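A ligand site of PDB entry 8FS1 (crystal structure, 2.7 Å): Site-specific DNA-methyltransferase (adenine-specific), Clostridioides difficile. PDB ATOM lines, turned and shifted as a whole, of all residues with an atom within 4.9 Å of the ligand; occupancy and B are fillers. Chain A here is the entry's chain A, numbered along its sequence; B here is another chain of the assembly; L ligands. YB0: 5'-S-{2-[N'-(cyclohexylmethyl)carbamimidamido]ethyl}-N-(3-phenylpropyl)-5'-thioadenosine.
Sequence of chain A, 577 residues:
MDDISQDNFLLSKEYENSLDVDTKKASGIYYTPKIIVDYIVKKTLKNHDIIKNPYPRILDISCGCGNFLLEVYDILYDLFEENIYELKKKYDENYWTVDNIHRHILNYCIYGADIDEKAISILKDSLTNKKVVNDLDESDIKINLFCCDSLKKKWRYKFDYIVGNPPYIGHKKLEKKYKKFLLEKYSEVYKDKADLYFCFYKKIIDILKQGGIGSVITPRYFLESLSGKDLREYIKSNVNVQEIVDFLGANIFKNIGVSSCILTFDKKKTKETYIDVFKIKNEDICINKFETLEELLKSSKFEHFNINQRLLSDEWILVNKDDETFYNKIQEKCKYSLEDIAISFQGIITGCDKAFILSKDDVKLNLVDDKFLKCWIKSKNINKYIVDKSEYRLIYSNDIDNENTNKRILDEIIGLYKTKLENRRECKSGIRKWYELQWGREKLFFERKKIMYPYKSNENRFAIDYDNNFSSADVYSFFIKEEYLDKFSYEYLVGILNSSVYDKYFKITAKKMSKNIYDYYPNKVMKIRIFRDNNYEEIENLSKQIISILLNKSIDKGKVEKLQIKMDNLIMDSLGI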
ATOM      1  N   TYR A  30      18.414 -29.660 -18.048  1.00  0.00           N
ATOM      2  CA  TYR A  30      17.267 -29.275 -18.867  1.00  0.00           C
ATOM      3  C   TYR A  30      16.938 -30.338 -19.917  1.00  0.00           C
ATOM      4  O   TYR A  30      16.040 -30.156 -20.741  1.00  0.00           O
ATOM      5  CB  TYR A  30      17.500 -27.925 -19.548  1.00  0.00           C
ATOM      6  CG  TYR A  30      17.880 -26.805 -18.592  1.00  0.00           C
ATOM      7  CD1 TYR A  30      16.923 -26.193 -17.789  1.00  0.00           C
ATOM      8  CD2 TYR A  30      19.189 -26.364 -18.490  1.00  0.00           C
ATOM      9  CE1 TYR A  30      17.260 -25.177 -16.918  1.00  0.00           C
ATOM     10  CE2 TYR A  30      19.542 -25.343 -17.620  1.00  0.00           C
ATOM     11  CZ  TYR A  30      18.573 -24.755 -16.832  1.00  0.00           C
ATOM     12  OH  TYR A  30      18.910 -23.739 -15.960  1.00  0.00           O
ATOM     13  N   ILE A  61      12.723 -25.425 -32.563  1.00  0.00           N
ATOM     14  CA  ILE A  61      13.221 -24.053 -32.531  1.00  0.00           C
ATOM     15  C   ILE A  61      14.240 -23.797 -31.440  1.00  0.00           C
ATOM     16  O   ILE A  61      14.966 -22.800 -31.509  1.00  0.00           O
ATOM     17  CB  ILE A  61      11.972 -23.157 -32.427  1.00  0.00           C
ATOM     18  CG1 ILE A  61      11.653 -22.484 -33.743  1.00  0.00           C
ATOM     19  CG2 ILE A  61      12.108 -22.117 -31.354  1.00  0.00           C
ATOM     20  CD1 ILE A  61      10.583 -21.423 -33.593  1.00  0.00           C
ATOM     21  N   SER A  62      14.365 -24.696 -30.471  1.00  0.00           N
ATOM     22  CA  SER A  62      15.364 -24.622 -29.420  1.00  0.00           C
ATOM     23  C   SER A  62      15.972 -26.012 -29.207  1.00  0.00           C
ATOM     24  O   SER A  62      15.982 -26.551 -28.096  1.00  0.00           O
ATOM     25  CB  SER A  62      14.752 -24.077 -28.133  1.00  0.00           C
ATOM     26  OG  SER A  62      13.623 -24.849 -27.765  1.00  0.00           O
ATOM     27  N   GLY A  64      18.749 -27.629 -29.007  1.00  0.00           N
ATOM     28  CA  GLY A  64      19.838 -28.065 -28.142  1.00  0.00           C
ATOM     29  C   GLY A  64      20.676 -29.144 -28.809  1.00  0.00           C
ATOM     30  O   GLY A  64      21.051 -29.039 -29.984  1.00  0.00           O
ATOM     31  N   ALA A 113      17.046 -25.256 -34.833  1.00  0.00           N
ATOM     32  CA  ALA A 113      17.630 -23.948 -34.555  1.00  0.00           C
ATOM     33  C   ALA A 113      18.004 -23.881 -33.085  1.00  0.00           C
ATOM     34  O   ALA A 113      17.290 -24.425 -32.232  1.00  0.00           O
ATOM     35  CB  ALA A 113      16.652 -22.809 -34.897  1.00  0.00           C
ATOM     36  N   ASP A 114      19.110 -23.202 -32.801  1.00  0.00           N
ATOM     37  CA  ASP A 114      19.534 -23.019 -31.416  1.00  0.00           C
ATOM     38  C   ASP A 114      20.551 -21.895 -31.360  1.00  0.00           C
ATOM     39  O   ASP A 114      21.324 -21.679 -32.301  1.00  0.00           O
ATOM     40  CB  ASP A 114      20.133 -24.294 -30.823  1.00  0.00           C
ATOM     41  CG  ASP A 114      20.082 -24.301 -29.316  1.00  0.00           C
ATOM     42  OD1 ASP A 114      20.791 -23.462 -28.694  1.00  0.00           O
ATOM     43  OD2 ASP A 114      19.309 -25.114 -28.744  1.00  0.00           O
ATOM     44  N   ILE A 115      20.552 -21.175 -30.237  1.00  0.00           N
ATOM     45  CA  ILE A 115      21.478 -20.065 -30.067  1.00  0.00           C
ATOM     46  C   ILE A 115      22.877 -20.535 -29.680  1.00  0.00           C
ATOM     47  O   ILE A 115      23.844 -19.788 -29.880  1.00  0.00           O
ATOM     48  CB  ILE A 115      20.882 -19.080 -29.038  1.00  0.00           C
ATOM     49  CG1 ILE A 115      21.585 -17.724 -29.119  1.00  0.00           C
ATOM     50  CG2 ILE A 115      20.954 -19.640 -27.631  1.00  0.00           C
ATOM     51  CD1 ILE A 115      20.776 -16.656 -29.789  1.00  0.00           C
ATOM     52  N   ASP A 116      23.009 -21.764 -29.193  1.00  0.00           N
ATOM     53  CA  ASP A 116      24.287 -22.306 -28.717  1.00  0.00           C
ATOM     54  C   ASP A 116      24.977 -23.042 -29.856  1.00  0.00           C
ATOM     55  O   ASP A 116      24.538 -24.115 -30.281  1.00  0.00           O
ATOM     56  CB  ASP A 116      24.048 -23.259 -27.542  1.00  0.00           C
ATOM     57  CG  ASP A 116      25.346 -23.799 -26.961  1.00  0.00           C
ATOM     58  OD1 ASP A 116      26.422 -23.221 -27.237  1.00  0.00           O
ATOM     59  OD2 ASP A 116      25.287 -24.831 -26.253  1.00  0.00           O
ATOM     60  N   ALA A 119      26.069 -26.617 -29.166  1.00  0.00           N
ATOM     61  CA  ALA A 119      24.972 -27.568 -29.236  1.00  0.00           C
ATOM     62  C   ALA A 119      24.689 -27.974 -30.676  1.00  0.00           C
ATOM     63  O   ALA A 119      24.541 -29.153 -30.989  1.00  0.00           O
ATOM     64  CB  ALA A 119      23.719 -26.972 -28.592  1.00  0.00           C
ATOM     65  N   CYS A 148      21.209 -19.416 -34.297  1.00  0.00           N
ATOM     66  CA  CYS A 148      20.566 -18.111 -34.323  1.00  0.00           C
ATOM     67  C   CYS A 148      19.634 -17.968 -33.121  1.00  0.00           C
ATOM     68  O   CYS A 148      19.372 -18.922 -32.384  1.00  0.00           O
ATOM     69  CB  CYS A 148      19.760 -17.917 -35.614  1.00  0.00           C
ATOM     70  SG  CYS A 148      18.330 -19.035 -35.752  1.00  0.00           S
ATOM     71  N   ASP A 149      19.117 -16.747 -32.959  1.00  0.00           N
ATOM     72  CA  ASP A 149      18.010 -16.460 -32.067  1.00  0.00           C
ATOM     73  C   ASP A 149      16.725 -16.753 -32.825  1.00  0.00           C
ATOM     74  O   ASP A 149      16.392 -16.062 -33.787  1.00  0.00           O
ATOM     75  CB  ASP A 149      18.066 -15.004 -31.619  1.00  0.00           C
ATOM     76  CG  ASP A 149      16.959 -14.625 -30.647  1.00  0.00           C
ATOM     77  OD1 ASP A 149      15.925 -15.330 -30.549  1.00  0.00           O
ATOM     78  OD2 ASP A 149      17.116 -13.568 -29.995  1.00  0.00           O
ATOM     79  N   SER A 150      15.990 -17.777 -32.392  1.00  0.00           N
ATOM     80  CA  SER A 150      14.792 -18.158 -33.136  1.00  0.00           C
ATOM     81  C   SER A 150      13.773 -17.027 -33.183  1.00  0.00           C
ATOM     82  O   SER A 150      13.013 -16.908 -34.159  1.00  0.00           O
ATOM     83  CB  SER A 150      14.172 -19.414 -32.516  1.00  0.00           C
ATOM     84  OG  SER A 150      15.041 -20.514 -32.653  1.00  0.00           O
ATOM     85  N   LEU A 151      13.739 -16.179 -32.161  1.00  0.00           N
ATOM     86  CA  LEU A 151      12.772 -15.090 -32.137  1.00  0.00           C
ATOM     87  C   LEU A 151      13.141 -13.969 -33.090  1.00  0.00           C
ATOM     88  O   LEU A 151      12.297 -13.118 -33.395  1.00  0.00           O
ATOM     89  CB  LEU A 151      12.621 -14.569 -30.715  1.00  0.00           C
ATOM     90  CG  LEU A 151      12.251 -15.653 -29.678  1.00  0.00           C
ATOM     91  CD1 LEU A 151      11.975 -15.016 -28.326  1.00  0.00           C
ATOM     92  CD2 LEU A 151      11.083 -16.546 -30.142  1.00  0.00           C
ATOM     93  N   ASN A 165      11.224 -28.204 -26.516  1.00  0.00           N
ATOM     94  CA  ASN A 165      11.149 -27.717 -25.138  1.00  0.00           C
ATOM     95  C   ASN A 165      11.836 -26.352 -25.094  1.00  0.00           C
ATOM     96  O   ASN A 165      13.064 -26.275 -24.976  1.00  0.00           O
ATOM     97  CB  ASN A 165      11.828 -28.714 -24.191  1.00  0.00           C
ATOM     98  CG  ASN A 165      11.901 -28.230 -22.737  1.00  0.00           C
ATOM     99  OD1 ASN A 165      11.150 -27.366 -22.304  1.00  0.00           O
ATOM    100  ND2 ASN A 165      12.826 -28.820 -21.988  1.00  0.00           N
ATOM    101  N   PRO A 166      11.072 -25.259 -25.176  1.00  0.00           N
ATOM    102  CA  PRO A 166      11.668 -23.910 -25.327  1.00  0.00           C
ATOM    103  C   PRO A 166      12.308 -23.434 -24.032  1.00  0.00           C
ATOM    104  O   PRO A 166      12.093 -24.024 -22.974  1.00  0.00           O
ATOM    105  CB  PRO A 166      10.463 -23.039 -25.693  1.00  0.00           C
ATOM    106  CG  PRO A 166       9.323 -23.708 -25.010  1.00  0.00           C
ATOM    107  CD  PRO A 166       9.603 -25.204 -25.135  1.00  0.00           C
ATOM    108  N   PRO A 167      13.109 -22.369 -24.085  1.00  0.00           N
ATOM    109  CA  PRO A 167      13.643 -21.775 -22.839  1.00  0.00           C
ATOM    110  C   PRO A 167      12.566 -21.066 -22.039  1.00  0.00           C
ATOM    111  O   PRO A 167      11.654 -20.453 -22.607  1.00  0.00           O
ATOM    112  CB  PRO A 167      14.709 -20.785 -23.349  1.00  0.00           C
ATOM    113  CG  PRO A 167      14.216 -20.398 -24.705  1.00  0.00           C
ATOM    114  CD  PRO A 167      13.619 -21.669 -25.283  1.00  0.00           C
ATOM    115  N   TYR A 168      12.666 -21.162 -20.710  1.00  0.00           N
ATOM    116  CA  TYR A 168      11.812 -20.428 -19.775  1.00  0.00           C
ATOM    117  C   TYR A 168      12.668 -19.387 -19.040  1.00  0.00           C
ATOM    118  O   TYR A 168      13.628 -19.758 -18.347  1.00  0.00           O
ATOM    119  CB  TYR A 168      11.157 -21.344 -18.730  1.00  0.00           C
ATOM    120  CG  TYR A 168      10.829 -22.780 -19.123  1.00  0.00           C
ATOM    121  CD1 TYR A 168      10.523 -23.143 -20.428  1.00  0.00           C
ATOM    122  CD2 TYR A 168      10.783 -23.768 -18.144  1.00  0.00           C
ATOM    123  CE1 TYR A 168      10.219 -24.461 -20.766  1.00  0.00           C
ATOM    124  CE2 TYR A 168      10.475 -25.089 -18.473  1.00  0.00           C
ATOM    125  CZ  TYR A 168      10.197 -25.427 -19.779  1.00  0.00           C
ATOM    126  OH  TYR A 168       9.893 -26.740 -20.103  1.00  0.00           O
ATOM    127  N   ILE A 169      12.355 -18.111 -19.213  1.00  0.00           N
ATOM    128  CA  ILE A 169      13.077 -17.042 -18.501  1.00  0.00           C
ATOM    129  C   ILE A 169      12.078 -15.990 -18.058  1.00  0.00           C
ATOM    130  O   ILE A 169      11.425 -15.355 -18.886  1.00  0.00           O
ATOM    131  CB  ILE A 169      14.179 -16.393 -19.353  1.00  0.00           C
ATOM    132  CG1 ILE A 169      15.099 -17.464 -19.951  1.00  0.00           C
ATOM    133  CG2 ILE A 169      14.970 -15.430 -18.479  1.00  0.00           C
ATOM    134  CD1 ILE A 169      16.124 -16.936 -20.897  1.00  0.00           C
ATOM    135  N   GLU A 175      17.337 -10.426 -19.739  1.00  0.00           N
ATOM    136  CA  GLU A 175      18.163  -9.239 -19.948  1.00  0.00           C
ATOM    137  C   GLU A 175      17.279  -8.047 -20.328  1.00  0.00           C
ATOM    138  O   GLU A 175      16.395  -8.174 -21.173  1.00  0.00           O
ATOM    139  CB  GLU A 175      19.207  -9.519 -21.034  1.00  0.00           C
ATOM    140  CG  GLU A 175      20.255  -8.441 -21.239  1.00  0.00           C
ATOM    141  CD  GLU A 175      21.268  -8.785 -22.318  1.00  0.00           C
ATOM    142  OE1 GLU A 175      21.309  -9.965 -22.735  1.00  0.00           O
ATOM    143  OE2 GLU A 175      22.022  -7.884 -22.750  1.00  0.00           O
ATOM    144  N   TYR A 178      17.170  -6.975 -23.945  1.00  0.00           N
ATOM    145  CA  TYR A 178      16.389  -7.916 -24.759  1.00  0.00           C
ATOM    146  C   TYR A 178      14.895  -7.706 -24.579  1.00  0.00           C
ATOM    147  O   TYR A 178      14.126  -7.873 -25.533  1.00  0.00           O
ATOM    148  CB  TYR A 178      16.767  -9.350 -24.396  1.00  0.00           C
ATOM    149  CG  TYR A 178      16.333 -10.381 -25.395  1.00  0.00           C
ATOM    150  CD1 TYR A 178      17.093 -10.648 -26.529  1.00  0.00           C
ATOM    151  CD2 TYR A 178      15.145 -11.088 -25.235  1.00  0.00           C
ATOM    152  CE1 TYR A 178      16.692 -11.599 -27.457  1.00  0.00           C
ATOM    153  CE2 TYR A 178      14.736 -12.045 -26.146  1.00  0.00           C
ATOM    154  CZ  TYR A 178      15.515 -12.293 -27.264  1.00  0.00           C
ATOM    155  OH  TYR A 178      15.122 -13.228 -28.183  1.00  0.00           O
ATOM    156  N   LEU A 196       9.516 -15.499 -21.295  1.00  0.00           N
ATOM    157  CA  LEU A 196      10.074 -15.658 -22.636  1.00  0.00           C
ATOM    158  C   LEU A 196       9.372 -16.750 -23.429  1.00  0.00           C
ATOM    159  O   LEU A 196       9.110 -16.581 -24.626  1.00  0.00           O
ATOM    160  CB  LEU A 196      11.563 -15.977 -22.527  1.00  0.00           C
ATOM    161  CG  LEU A 196      12.294 -16.321 -23.822  1.00  0.00           C
ATOM    162  CD1 LEU A 196      12.322 -15.125 -24.735  1.00  0.00           C
ATOM    163  CD2 LEU A 196      13.691 -16.786 -23.505  1.00  0.00           C
ATOM    164  N   PHE A 200       7.887 -18.016 -27.608  1.00  0.00           N
ATOM    165  CA  PHE A 200       8.115 -19.211 -28.418  1.00  0.00           C
ATOM    166  C   PHE A 200       6.790 -19.827 -28.863  1.00  0.00           C
ATOM    167  O   PHE A 200       6.687 -20.275 -30.000  1.00  0.00           O
ATOM    168  CB  PHE A 200       8.984 -20.201 -27.654  1.00  0.00           C
ATOM    169  CG  PHE A 200      10.447 -19.854 -27.707  1.00  0.00           C
ATOM    170  CD1 PHE A 200      10.947 -18.807 -26.952  1.00  0.00           C
ATOM    171  CD2 PHE A 200      11.293 -20.542 -28.547  1.00  0.00           C
ATOM    172  CE1 PHE A 200      12.289 -18.484 -27.017  1.00  0.00           C
ATOM    173  CE2 PHE A 200      12.630 -20.209 -28.623  1.00  0.00           C
ATOM    174  CZ  PHE A 200      13.126 -19.182 -27.854  1.00  0.00           C
ATOM    175  P    DA B   8      11.599 -18.981 -12.377  1.00  0.00           P
ATOM    176  OP1  DA B   8      12.852 -18.671 -11.642  1.00  0.00           O
ATOM    177  OP2  DA B   8      11.196 -18.220 -13.587  1.00  0.00           O
ATOM    178  O5'  DA B   8      11.640 -20.512 -12.779  1.00  0.00           O
ATOM    179  C5'  DA B   8      12.246 -20.910 -13.969  1.00  0.00           C
ATOM    180  C4'  DA B   8      12.722 -22.329 -13.834  1.00  0.00           C
ATOM    181  O4'  DA B   8      12.530 -23.042 -15.089  1.00  0.00           O
ATOM    182  C3'  DA B   8      14.198 -22.486 -13.484  1.00  0.00           C
ATOM    183  O3'  DA B   8      14.348 -23.540 -12.570  1.00  0.00           O
ATOM    184  C2'  DA B   8      14.825 -22.825 -14.831  1.00  0.00           C
ATOM    185  C1'  DA B   8      13.727 -23.690 -15.438  1.00  0.00           C
ATOM    186  N9   DA B   8      13.787 -23.851 -16.884  1.00  0.00           N
ATOM    187  C8   DA B   8      14.032 -22.875 -17.811  1.00  0.00           C
ATOM    188  N7   DA B   8      14.026 -23.310 -19.047  1.00  0.00           N
ATOM    189  C5   DA B   8      13.787 -24.669 -18.928  1.00  0.00           C
ATOM    190  C6   DA B   8      13.663 -25.713 -19.878  1.00  0.00           C
ATOM    191  N6   DA B   8      13.777 -25.525 -21.193  1.00  0.00           N
ATOM    192  N1   DA B   8      13.404 -26.954 -19.420  1.00  0.00           N
ATOM    193  C2   DA B   8      13.278 -27.139 -18.098  1.00  0.00           C
ATOM    194  N3   DA B   8      13.371 -26.242 -17.111  1.00  0.00           N
ATOM    195  C4   DA B   8      13.639 -25.016 -17.594  1.00  0.00           C
HETATM  196  C5  YB0 L   1      17.805 -24.709 -25.485  1.00  0.00           C
HETATM  197  C6  YB0 L   1      17.079 -25.221 -24.260  1.00  0.00           C
HETATM  198  C8  YB0 L   1      17.448 -23.940 -21.728  1.00  0.00           C
HETATM  199  N12 YB0 L   1      18.152 -20.855 -20.061  1.00  0.00           N
HETATM  200  C13 YB0 L   1      18.870 -19.595 -19.849  1.00  0.00           C
HETATM  201  C15 YB0 L   1      20.924 -20.539 -20.962  1.00  0.00           C
HETATM  202  C17 YB0 L   1      21.516 -19.880 -23.326  1.00  0.00           C
HETATM  203  C22 YB0 L   1      18.255 -22.732 -26.537  1.00  0.00           C
HETATM  204  C24 YB0 L   1      17.561 -20.443 -25.689  1.00  0.00           C
HETATM  205  C26 YB0 L   1      17.100 -19.429 -27.499  1.00  0.00           C
HETATM  206  C11 YB0 L   1      18.112 -21.822 -19.142  1.00  0.00           C
HETATM  207  C14 YB0 L   1      19.953 -19.361 -20.896  1.00  0.00           C
HETATM  208  C16 YB0 L   1      21.140 -21.022 -22.396  1.00  0.00           C
HETATM  209  C18 YB0 L   1      20.447 -18.800 -23.310  1.00  0.00           C
HETATM  210  C19 YB0 L   1      19.365 -19.093 -22.273  1.00  0.00           C
HETATM  211  C2  YB0 L   1      19.271 -24.386 -25.168  1.00  0.00           C
HETATM  212  C27 YB0 L   1      17.520 -20.698 -27.859  1.00  0.00           C
HETATM  213  C29 YB0 L   1      17.250 -20.276 -30.009  1.00  0.00           C
HETATM  214  C3  YB0 L   1      19.439 -22.915 -25.601  1.00  0.00           C
HETATM  215  C31 YB0 L   1      16.723 -18.566 -28.564  1.00  0.00           C
HETATM  216  C33 YB0 L   1      16.009 -16.671 -27.113  1.00  0.00           C
HETATM  217  C34 YB0 L   1      17.245 -15.921 -26.653  1.00  0.00           C
HETATM  218  C35 YB0 L   1      17.037 -15.237 -25.308  1.00  0.00           C
HETATM  219  C36 YB0 L   1      18.304 -14.668 -24.720  1.00  0.00           C
HETATM  220  C37 YB0 L   1      19.208 -15.503 -24.071  1.00  0.00           C
HETATM  221  C38 YB0 L   1      20.357 -14.970 -23.498  1.00  0.00           C
HETATM  222  C39 YB0 L   1      20.611 -13.623 -23.566  1.00  0.00           C
HETATM  223  C40 YB0 L   1      19.714 -12.788 -24.200  1.00  0.00           C
HETATM  224  C41 YB0 L   1      18.573 -13.310 -24.776  1.00  0.00           C
HETATM  225  C9  YB0 L   1      16.707 -23.119 -20.691  1.00  0.00           C
HETATM  226  N10 YB0 L   1      17.435 -22.939 -19.434  1.00  0.00           N
HETATM  227  N20 YB0 L   1      18.698 -21.667 -18.004  1.00  0.00           N
HETATM  228  N23 YB0 L   1      17.811 -21.339 -26.676  1.00  0.00           N
HETATM  229  N25 YB0 L   1      17.129 -19.272 -26.116  1.00  0.00           N
HETATM  230  N28 YB0 L   1      17.618 -21.182 -29.094  1.00  0.00           N
HETATM  231  N30 YB0 L   1      16.817 -19.026 -29.816  1.00  0.00           N
HETATM  232  N32 YB0 L   1      16.241 -17.322 -28.387  1.00  0.00           N
HETATM  233  O1  YB0 L   1      20.142 -25.296 -25.827  1.00  0.00           O
HETATM  234  O21 YB0 L   1      17.207 -23.483 -25.977  1.00  0.00           O
HETATM  235  O4  YB0 L   1      20.640 -22.680 -26.326  1.00  0.00           O
HETATM  236  S7  YB0 L   1      16.539 -23.797 -23.292  1.00  0.00           S
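An oxygen (O4) of the ligand is in hydrogen-bond range of the side-chain carboxylate (OD1) of Asp 114 (2.5 Å).
N20 of the ligand sits at hydrogen-bond distance from OH of Tyr 30, 2.9 Å away.
OD1 of Asp 149 is in hydrogen-bond range of N32 of the ligand, 3.0 Å away.
N30 of the ligand lies within hydrogen-bond range of N of Ser 150 (3.0 Å).
The backbone NH of Ile 115 lies within hydrogen-bond range of a nitrogen (N28) of the ligand (3.1 Å).
N7 of DA 8 of chain B sits close to a nitrogen (N10) of the ligand (3.5 Å).
The backbone NH (N) of Gly 64 lies within hydrogen-bond range of the side-chain carboxylate (OD2) of Asp 114.
The side-chain carboxylate (OD1) of Asp 114 is in hydrogen-bond range of the backbone NH (N) of Asp 116 (2.8 Å).
N of Leu 151 lies within hydrogen-bond range of OD1 of Asp 149, 2.8 Å away.
O of Cys 148 lies within hydrogen-bond range of N of Ile 115 (3.3 Å).
N1 of DA 8 of chain B lies within hydrogen-bond range of the side-chain amide nitrogen of Asn 165 (3.2 Å).
N7 of DA 8 of chain B is in hydrogen-bond range of N of Tyr 168.
The backbone NH (N) of Ser 62 lies close to the backbone carbonyl oxygen (O) of Ala 113, 3.4 Å away.
O of Ile 169 lies within hydrogen-bond range of N of Leu 196 (3.1 Å).
A sulfur (S7) of the ligand lies close to the backbone nitrogen (N) of Pro 167 (3.8 Å).
Merely in contact with the ligand: Ser 62 (3.3 Å), Cys 148 (3.5 Å), Tyr 178 (3.5 Å), Glu 175 (3.6 Å), Gly 64 (3.6 Å), Asp 116 (3.7 Å), Phe 200 (3.7 Å), Ile 61 (3.7 Å) and Ile 169 (3.96 Å).
Hydrophobic or aromatic side chains within 4 Å of the ligand: Tyr 30, Ile 115, Pro 167, Ile 169, Tyr 178 and Phe 200.
Of the 23 residues printed, 16 come within 4 Å of the ligand.
Along chain A the residues within 4 Å of the ligand span positions 30 to 200.
The nearest printed residue that does not touch the ligand is Leu 196 (4.1 Å).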
